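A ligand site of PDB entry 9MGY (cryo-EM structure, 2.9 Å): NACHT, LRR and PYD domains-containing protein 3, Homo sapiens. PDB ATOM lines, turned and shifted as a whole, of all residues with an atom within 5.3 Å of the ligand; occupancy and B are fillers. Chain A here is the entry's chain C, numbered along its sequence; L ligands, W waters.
The side-chain hydroxyl (OH) of Tyr 443 sits close to a fluorine (F3) of the ligand.
CB of Ala 227 touches O1 of the ligand (3.2 Å).
Ile 411 touches the ligand (CD1 to C17, 3.4 Å).
Leu 413 touches the ligand (CD2 to F2, 3.5 Å).
Val 414 touches the ligand (CG2 to F1, 3.4 Å).
CG2 of Thr 439 touches F1 of the ligand, 3.0 Å away.
CD1 of Ile 574 touches C10 of the ligand (3.9 Å).
CZ of Phe 575 touches C17 of the ligand, 3.8 Å away.
Gln 624 touches the ligand (NE2 to C11, 3.1 Å).
Tyr 632 touches the ligand (CE1 to C2, 3.7 Å).
Met 661 touches the ligand.
Hydrophobic or aromatic side chains that line the ligand: Ala 227, Ala 228, Ile 411, Leu 413, Val 414, Tyr 443, Ile 574, Phe 575, Tyr 632 and Met 661.
14 residues have an atom within 4 Å of the ligand: Ala 227, Ala 228, Ile 411, Leu 413, Val 414, Thr 439, Tyr 443, Ile 574, Phe 575, Arg 578, Gln 624, Glu 629, Tyr 632 and Met 661.
The guanidinium group (NH2) of Arg 578 is in salt-bridge range of the side-chain carboxylate (OE1) of Glu 629 (2.7 Å).
OG of Ser 626 sits at hydrogen-bond distance from N of Glu 629 (3.3 Å).
The side-chain hydroxyl (OH) of Tyr 443 is in hydrogen-bond range of the side-chain hydroxyl (OG1) of Thr 524 (2.6 Å).
The side-chain amide nitrogen (NE2) of Gln 624 lies within hydrogen-bond range of the side-chain hydroxyl (OG) of Ser 626 (3.2 Å).
The side-chain hydroxyl (OH) of Tyr 632 is in hydrogen-bond range of the side-chain carboxylate (OD1) of Asp 662 (2.5 Å).
The backbone NH (N) of Ala 228 lies within hydrogen-bond range of an oxygen (O1) of the ligand, 3.3 Å away.
The backbone carbonyl oxygen (O) of Ala 228 sits at hydrogen-bond distance from an oxygen (O1) of the ligand, 2.6 Å away.
The guanidinium group (NH1) of Arg 578 sits at hydrogen-bond distance from a nitrogen (N2) of the ligand (2.6 Å).
N1 of the ligand lies within salt-bridge range of OE1 of Glu 629, 2.7 Å away.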
ATOM      1  N   ALA A 227      28.633   5.654   7.105  1.00  0.00           N
ATOM      2  CA  ALA A 227      27.870   6.707   7.718  1.00  0.00           C
ATOM      3  C   ALA A 227      26.435   6.343   7.854  1.00  0.00           C
ATOM      4  O   ALA A 227      25.993   5.445   7.214  1.00  0.00           O
ATOM      5  CB  ALA A 227      28.016   7.809   6.750  1.00  0.00           C
ATOM      6  N   ALA A 228      25.731   7.118   8.641  1.00  0.00           N
ATOM      7  CA  ALA A 228      24.293   6.946   8.811  1.00  0.00           C
ATOM      8  C   ALA A 228      23.609   7.296   7.522  1.00  0.00           C
ATOM      9  O   ALA A 228      23.626   8.446   7.174  1.00  0.00           O
ATOM     10  CB  ALA A 228      23.953   7.942   9.830  1.00  0.00           C
ATOM     11  N   GLY A 229      23.025   6.336   6.840  1.00  0.00           N
ATOM     12  CA  GLY A 229      22.285   6.577   5.596  1.00  0.00           C
ATOM     13  C   GLY A 229      22.995   6.040   4.405  1.00  0.00           C
ATOM     14  O   GLY A 229      22.390   5.961   3.408  1.00  0.00           O
ATOM     15  N   ARG A 351      28.446   1.981  12.340  1.00  0.00           N
ATOM     16  CA  ARG A 351      28.983   3.324  12.131  1.00  0.00           C
ATOM     17  C   ARG A 351      30.424   3.356  12.645  1.00  0.00           C
ATOM     18  O   ARG A 351      30.684   2.808  13.711  1.00  0.00           O
ATOM     19  CB  ARG A 351      28.154   4.367  12.861  1.00  0.00           C
ATOM     20  CG  ARG A 351      26.766   4.567  12.321  1.00  0.00           C
ATOM     21  CD  ARG A 351      25.989   5.500  13.154  1.00  0.00           C
ATOM     22  NE  ARG A 351      26.502   6.847  13.053  1.00  0.00           N
ATOM     23  CZ  ARG A 351      26.244   7.840  13.921  1.00  0.00           C
ATOM     24  NH1 ARG A 351      25.489   7.629  14.966  1.00  0.00           N
ATOM     25  NH2 ARG A 351      26.770   9.026  13.712  1.00  0.00           N
ATOM     26  N   PHE A 410      25.323  12.222  -2.161  1.00  0.00           N
ATOM     27  CA  PHE A 410      26.071  10.969  -2.282  1.00  0.00           C
ATOM     28  C   PHE A 410      25.510   9.953  -1.305  1.00  0.00           C
ATOM     29  O   PHE A 410      25.648   8.749  -1.504  1.00  0.00           O
ATOM     30  CB  PHE A 410      27.570  11.175  -2.062  1.00  0.00           C
ATOM     31  CG  PHE A 410      28.051  11.148  -0.651  1.00  0.00           C
ATOM     32  CD1 PHE A 410      28.508   9.975  -0.074  1.00  0.00           C
ATOM     33  CD2 PHE A 410      28.075  12.289   0.119  1.00  0.00           C
ATOM     34  CE1 PHE A 410      28.971   9.946   1.214  1.00  0.00           C
ATOM     35  CE2 PHE A 410      28.534  12.269   1.404  1.00  0.00           C
ATOM     36  CZ  PHE A 410      28.976  11.097   1.955  1.00  0.00           C
ATOM     37  N   ILE A 411      24.863  10.440  -0.248  1.00  0.00           N
ATOM     38  CA  ILE A 411      24.239   9.587   0.734  1.00  0.00           C
ATOM     39  C   ILE A 411      22.820   9.214   0.271  1.00  0.00           C
ATOM     40  O   ILE A 411      21.967  10.092   0.159  1.00  0.00           O
ATOM     41  CB  ILE A 411      24.160  10.307   2.083  1.00  0.00           C
ATOM     42  CG1 ILE A 411      25.560  10.650   2.542  1.00  0.00           C
ATOM     43  CG2 ILE A 411      23.465   9.437   3.105  1.00  0.00           C
ATOM     44  CD1 ILE A 411      25.624  11.635   3.670  1.00  0.00           C
ATOM     45  N   LEU A 413      20.255   8.133   1.668  1.00  0.00           N
ATOM     46  CA  LEU A 413      19.201   8.707   2.482  1.00  0.00           C
ATOM     47  C   LEU A 413      18.871  10.126   2.063  1.00  0.00           C
ATOM     48  O   LEU A 413      17.707  10.522   2.071  1.00  0.00           O
ATOM     49  CB  LEU A 413      19.581   8.680   3.964  1.00  0.00           C
ATOM     50  CG  LEU A 413      18.550   9.267   4.944  1.00  0.00           C
ATOM     51  CD1 LEU A 413      17.242   8.509   4.864  1.00  0.00           C
ATOM     52  CD2 LEU A 413      19.130   9.199   6.351  1.00  0.00           C
ATOM     53  N   VAL A 414      19.885  10.895   1.712  1.00  0.00           N
ATOM     54  CA  VAL A 414      19.647  12.276   1.307  1.00  0.00           C
ATOM     55  C   VAL A 414      18.865  12.283   0.018  1.00  0.00           C
ATOM     56  O   VAL A 414      17.928  13.053  -0.145  1.00  0.00           O
ATOM     57  CB  VAL A 414      20.966  13.040   1.157  1.00  0.00           C
ATOM     58  CG1 VAL A 414      20.716  14.427   0.556  1.00  0.00           C
ATOM     59  CG2 VAL A 414      21.619  13.174   2.516  1.00  0.00           C
ATOM     60  N   ILE A 417      15.233  11.481   0.787  1.00  0.00           N
ATOM     61  CA  ILE A 417      14.539  12.587   1.430  1.00  0.00           C
ATOM     62  C   ILE A 417      14.184  13.654   0.409  1.00  0.00           C
ATOM     63  O   ILE A 417      13.069  14.176   0.411  1.00  0.00           O
ATOM     64  CB  ILE A 417      15.388  13.211   2.554  1.00  0.00           C
ATOM     65  CG1 ILE A 417      15.556  12.214   3.717  1.00  0.00           C
ATOM     66  CG2 ILE A 417      14.720  14.459   3.055  1.00  0.00           C
ATOM     67  CD1 ILE A 417      16.597  12.625   4.737  1.00  0.00           C
ATOM     68  N   THR A 439      22.335  19.825   6.119  1.00  0.00           N
ATOM     69  CA  THR A 439      21.563  18.627   6.445  1.00  0.00           C
ATOM     70  C   THR A 439      20.298  19.016   7.173  1.00  0.00           C
ATOM     71  O   THR A 439      19.225  18.477   6.897  1.00  0.00           O
ATOM     72  CB  THR A 439      22.383  17.629   7.291  1.00  0.00           C
ATOM     73  OG1 THR A 439      23.532  17.196   6.559  1.00  0.00           O
ATOM     74  CG2 THR A 439      21.530  16.418   7.643  1.00  0.00           C
ATOM     75  N   TYR A 443      16.247  18.304   6.271  1.00  0.00           N
ATOM     76  CA  TYR A 443      15.288  17.678   7.169  1.00  0.00           C
ATOM     77  C   TYR A 443      14.117  18.598   7.485  1.00  0.00           C
ATOM     78  O   TYR A 443      12.970  18.136   7.527  1.00  0.00           O
ATOM     79  CB  TYR A 443      15.974  17.220   8.458  1.00  0.00           C
ATOM     80  CG  TYR A 443      16.652  15.882   8.320  1.00  0.00           C
ATOM     81  CD1 TYR A 443      17.610  15.685   7.352  1.00  0.00           C
ATOM     82  CD2 TYR A 443      16.309  14.843   9.172  1.00  0.00           C
ATOM     83  CE1 TYR A 443      18.221  14.466   7.222  1.00  0.00           C
ATOM     84  CE2 TYR A 443      16.923  13.623   9.033  1.00  0.00           C
ATOM     85  CZ  TYR A 443      17.878  13.435   8.063  1.00  0.00           C
ATOM     86  OH  TYR A 443      18.483  12.212   7.921  1.00  0.00           O
ATOM     87  N   THR A 524      18.326   8.948  12.161  1.00  0.00           N
ATOM     88  CA  THR A 524      18.621  10.371  12.031  1.00  0.00           C
ATOM     89  C   THR A 524      17.395  11.227  12.249  1.00  0.00           C
ATOM     90  O   THR A 524      17.503  12.363  12.709  1.00  0.00           O
ATOM     91  CB  THR A 524      19.208  10.706  10.651  1.00  0.00           C
ATOM     92  OG1 THR A 524      18.290  10.289   9.642  1.00  0.00           O
ATOM     93  CG2 THR A 524      20.552  10.038  10.445  1.00  0.00           C
ATOM     94  N   ILE A 574      25.503  12.262  17.947  1.00  0.00           N
ATOM     95  CA  ILE A 574      26.215  13.033  16.940  1.00  0.00           C
ATOM     96  C   ILE A 574      25.280  13.901  16.141  1.00  0.00           C
ATOM     97  O   ILE A 574      25.544  15.073  15.919  1.00  0.00           O
ATOM     98  CB  ILE A 574      27.029  12.119  16.033  1.00  0.00           C
ATOM     99  CG1 ILE A 574      28.168  11.527  16.843  1.00  0.00           C
ATOM    100  CG2 ILE A 574      27.555  12.885  14.824  1.00  0.00           C
ATOM    101  CD1 ILE A 574      28.841  10.352  16.220  1.00  0.00           C
ATOM    102  N   PHE A 575      24.169  13.315  15.720  1.00  0.00           N
ATOM    103  CA  PHE A 575      23.214  14.074  14.957  1.00  0.00           C
ATOM    104  C   PHE A 575      22.363  14.958  15.843  1.00  0.00           C
ATOM    105  O   PHE A 575      21.903  16.010  15.414  1.00  0.00           O
ATOM    106  CB  PHE A 575      22.357  13.150  14.113  1.00  0.00           C
ATOM    107  CG  PHE A 575      23.105  12.612  12.946  1.00  0.00           C
ATOM    108  CD1 PHE A 575      23.728  11.387  13.013  1.00  0.00           C
ATOM    109  CD2 PHE A 575      23.180  13.339  11.787  1.00  0.00           C
ATOM    110  CE1 PHE A 575      24.427  10.903  11.930  1.00  0.00           C
ATOM    111  CE2 PHE A 575      23.879  12.856  10.704  1.00  0.00           C
ATOM    112  CZ  PHE A 575      24.507  11.636  10.783  1.00  0.00           C
ATOM    113  N   ARG A 578      24.594  17.927  16.168  1.00  0.00           N
ATOM    114  CA  ARG A 578      24.763  18.524  14.852  1.00  0.00           C
ATOM    115  C   ARG A 578      23.498  19.250  14.411  1.00  0.00           C
ATOM    116  O   ARG A 578      23.569  20.356  13.873  1.00  0.00           O
ATOM    117  CB  ARG A 578      25.133  17.453  13.840  1.00  0.00           C
ATOM    118  CG  ARG A 578      25.511  17.965  12.477  1.00  0.00           C
ATOM    119  CD  ARG A 578      25.821  16.871  11.509  1.00  0.00           C
ATOM    120  NE  ARG A 578      27.040  16.154  11.827  1.00  0.00           N
ATOM    121  CZ  ARG A 578      27.503  15.092  11.133  1.00  0.00           C
ATOM    122  NH1 ARG A 578      26.840  14.664  10.086  1.00  0.00           N
ATOM    123  NH2 ARG A 578      28.628  14.489  11.482  1.00  0.00           N
ATOM    124  N   PHE A 579      22.334  18.669  14.682  1.00  0.00           N
ATOM    125  CA  PHE A 579      21.075  19.312  14.346  1.00  0.00           C
ATOM    126  C   PHE A 579      20.809  20.530  15.210  1.00  0.00           C
ATOM    127  O   PHE A 579      20.256  21.523  14.724  1.00  0.00           O
ATOM    128  CB  PHE A 579      19.900  18.338  14.439  1.00  0.00           C
ATOM    129  CG  PHE A 579      19.763  17.408  13.248  1.00  0.00           C
ATOM    130  CD1 PHE A 579      19.751  16.043  13.407  1.00  0.00           C
ATOM    131  CD2 PHE A 579      19.633  17.912  11.966  1.00  0.00           C
ATOM    132  CE1 PHE A 579      19.619  15.206  12.326  1.00  0.00           C
ATOM    133  CE2 PHE A 579      19.501  17.075  10.886  1.00  0.00           C
ATOM    134  CZ  PHE A 579      19.491  15.715  11.065  1.00  0.00           C
ATOM    135  N   GLN A 624      35.397  11.783  20.772  1.00  0.00           N
ATOM    136  CA  GLN A 624      35.041  12.402  19.507  1.00  0.00           C
ATOM    137  C   GLN A 624      34.244  13.642  19.507  1.00  0.00           C
ATOM    138  O   GLN A 624      33.291  13.589  20.225  1.00  0.00           O
ATOM    139  CB  GLN A 624      34.321  11.313  18.673  1.00  0.00           C
ATOM    140  CG  GLN A 624      33.481  11.844  17.526  1.00  0.00           C
ATOM    141  CD  GLN A 624      34.218  11.792  16.213  1.00  0.00           C
ATOM    142  OE1 GLN A 624      35.175  11.053  16.040  1.00  0.00           O
ATOM    143  NE2 GLN A 624      33.762  12.590  15.279  1.00  0.00           N
ATOM    144  N   SER A 626      35.883  15.301  16.876  1.00  0.00           N
ATOM    145  CA  SER A 626      37.177  15.359  16.147  1.00  0.00           C
ATOM    146  C   SER A 626      37.534  16.466  15.187  1.00  0.00           C
ATOM    147  O   SER A 626      38.261  16.094  14.263  1.00  0.00           O
ATOM    148  CB  SER A 626      37.239  14.162  15.327  1.00  0.00           C
ATOM    149  OG  SER A 626      36.276  14.256  14.286  1.00  0.00           O
ATOM    150  N   LEU A 628      37.141  17.553  12.421  1.00  0.00           N
ATOM    151  CA  LEU A 628      36.295  17.406  11.230  1.00  0.00           C
ATOM    152  C   LEU A 628      34.862  17.394  11.715  1.00  0.00           C
ATOM    153  O   LEU A 628      34.037  18.016  11.096  1.00  0.00           O
ATOM    154  CB  LEU A 628      36.626  16.126  10.468  1.00  0.00           C
ATOM    155  CG  LEU A 628      35.974  16.022   9.097  1.00  0.00           C
ATOM    156  CD1 LEU A 628      36.189  17.273   8.286  1.00  0.00           C
ATOM    157  CD2 LEU A 628      36.489  14.804   8.350  1.00  0.00           C
ATOM    158  N   GLU A 629      34.592  16.734  12.822  1.00  0.00           N
ATOM    159  CA  GLU A 629      33.239  16.752  13.405  1.00  0.00           C
ATOM    160  C   GLU A 629      32.825  18.118  13.908  1.00  0.00           C
ATOM    161  O   GLU A 629      31.732  18.483  13.613  1.00  0.00           O
ATOM    162  CB  GLU A 629      33.148  15.721  14.503  1.00  0.00           C
ATOM    163  CG  GLU A 629      31.743  15.525  15.047  1.00  0.00           C
ATOM    164  CD  GLU A 629      30.622  15.446  14.031  1.00  0.00           C
ATOM    165  OE1 GLU A 629      30.784  14.728  13.041  1.00  0.00           O
ATOM    166  OE2 GLU A 629      29.581  16.087  14.249  1.00  0.00           O
ATOM    167  N   TYR A 632      31.614  19.886  10.826  1.00  0.00           N
ATOM    168  CA  TYR A 632      30.300  19.496  10.304  1.00  0.00           C
ATOM    169  C   TYR A 632      29.268  20.196  11.157  1.00  0.00           C
ATOM    170  O   TYR A 632      28.249  20.504  10.628  1.00  0.00           O
ATOM    171  CB  TYR A 632      30.163  17.996  10.359  1.00  0.00           C
ATOM    172  CG  TYR A 632      30.602  17.196   9.174  1.00  0.00           C
ATOM    173  CD1 TYR A 632      31.853  16.636   9.116  1.00  0.00           C
ATOM    174  CD2 TYR A 632      29.712  16.960   8.147  1.00  0.00           C
ATOM    175  CE1 TYR A 632      32.242  15.883   8.027  1.00  0.00           C
ATOM    176  CE2 TYR A 632      30.093  16.203   7.055  1.00  0.00           C
ATOM    177  CZ  TYR A 632      31.355  15.669   6.998  1.00  0.00           C
ATOM    178  OH  TYR A 632      31.710  14.929   5.928  1.00  0.00           O
ATOM    179  N   MET A 661      32.156  15.712   0.602  1.00  0.00           N
ATOM    180  CA  MET A 661      31.457  16.458   1.638  1.00  0.00           C
ATOM    181  C   MET A 661      32.431  16.932   2.714  1.00  0.00           C
ATOM    182  O   MET A 661      32.250  18.015   3.270  1.00  0.00           O
ATOM    183  CB  MET A 661      30.346  15.618   2.228  1.00  0.00           C
ATOM    184  CG  MET A 661      29.516  16.326   3.265  1.00  0.00           C
ATOM    185  SD  MET A 661      28.066  15.393   3.758  1.00  0.00           S
ATOM    186  CE  MET A 661      28.773  14.032   4.684  1.00  0.00           C
ATOM    187  N   ASP A 662      33.461  16.134   2.986  1.00  0.00           N
ATOM    188  CA  ASP A 662      34.460  16.511   3.973  1.00  0.00           C
ATOM    189  C   ASP A 662      35.196  17.752   3.513  1.00  0.00           C
ATOM    190  O   ASP A 662      35.531  18.625   4.320  1.00  0.00           O
ATOM    191  CB  ASP A 662      35.501  15.391   4.152  1.00  0.00           C
ATOM    192  CG  ASP A 662      35.005  14.156   4.821  1.00  0.00           C
ATOM    193  OD1 ASP A 662      34.070  14.216   5.577  1.00  0.00           O
ATOM    194  OD2 ASP A 662      35.568  13.125   4.540  1.00  0.00           O
HETATM  195  N1  LIG L   1      31.713  12.355  12.196  1.00  0.00           N
HETATM  196  N2  LIG L   1      27.995  12.969   8.437  1.00  0.00           N
HETATM  197  C1  LIG L   1      33.331  12.731   9.818  1.00  0.00           C
HETATM  198  C2  LIG L   1      31.813  12.618   9.752  1.00  0.00           C
HETATM  199  C3  LIG L   1      31.300  11.772  10.921  1.00  0.00           C
HETATM  200  C4  LIG L   1      30.099  12.055   8.101  1.00  0.00           C
HETATM  201  C5  LIG L   1      29.634  11.285   7.049  1.00  0.00           C
HETATM  202  C6  LIG L   1      27.506  12.254   7.423  1.00  0.00           C
HETATM  203  C7  LIG L   1      24.136  13.839   6.876  1.00  0.00           C
HETATM  204  C8  LIG L   1      23.847  11.470   6.865  1.00  0.00           C
HETATM  205  C9  LIG L   1      21.839  12.904   6.536  1.00  0.00           C
HETATM  206  C10 LIG L   1      31.158  11.590  13.310  1.00  0.00           C
HETATM  207  O1  LIG L   1      25.692  10.036   7.170  1.00  0.00           O
HETATM  208  C11 LIG L   1      33.172  12.369  12.262  1.00  0.00           C
HETATM  209  N3  LIG L   1      31.385  12.034   8.493  1.00  0.00           N
HETATM  210  C12 LIG L   1      33.757  13.250  11.179  1.00  0.00           C
HETATM  211  N4  LIG L   1      29.295  12.885   8.764  1.00  0.00           N
HETATM  212  C13 LIG L   1      28.307  11.381   6.721  1.00  0.00           C
HETATM  213  C14 LIG L   1      26.048  12.416   7.171  1.00  0.00           C
HETATM  214  C15 LIG L   1      25.489  13.684   7.091  1.00  0.00           C
HETATM  215  C16 LIG L   1      23.304  12.740   6.769  1.00  0.00           C
HETATM  216  C17 LIG L   1      25.198  11.301   7.070  1.00  0.00           C
HETATM  217  F1  LIG L   1      21.555  13.995   5.845  1.00  0.00           F
HETATM  218  F2  LIG L   1      21.325  11.893   5.850  1.00  0.00           F
HETATM  219  F3  LIG L   1      21.138  12.981   7.657  1.00  0.00           F
HETATM  220  O   HOH W   1      32.988  10.828   5.698  1.00  0.00           O
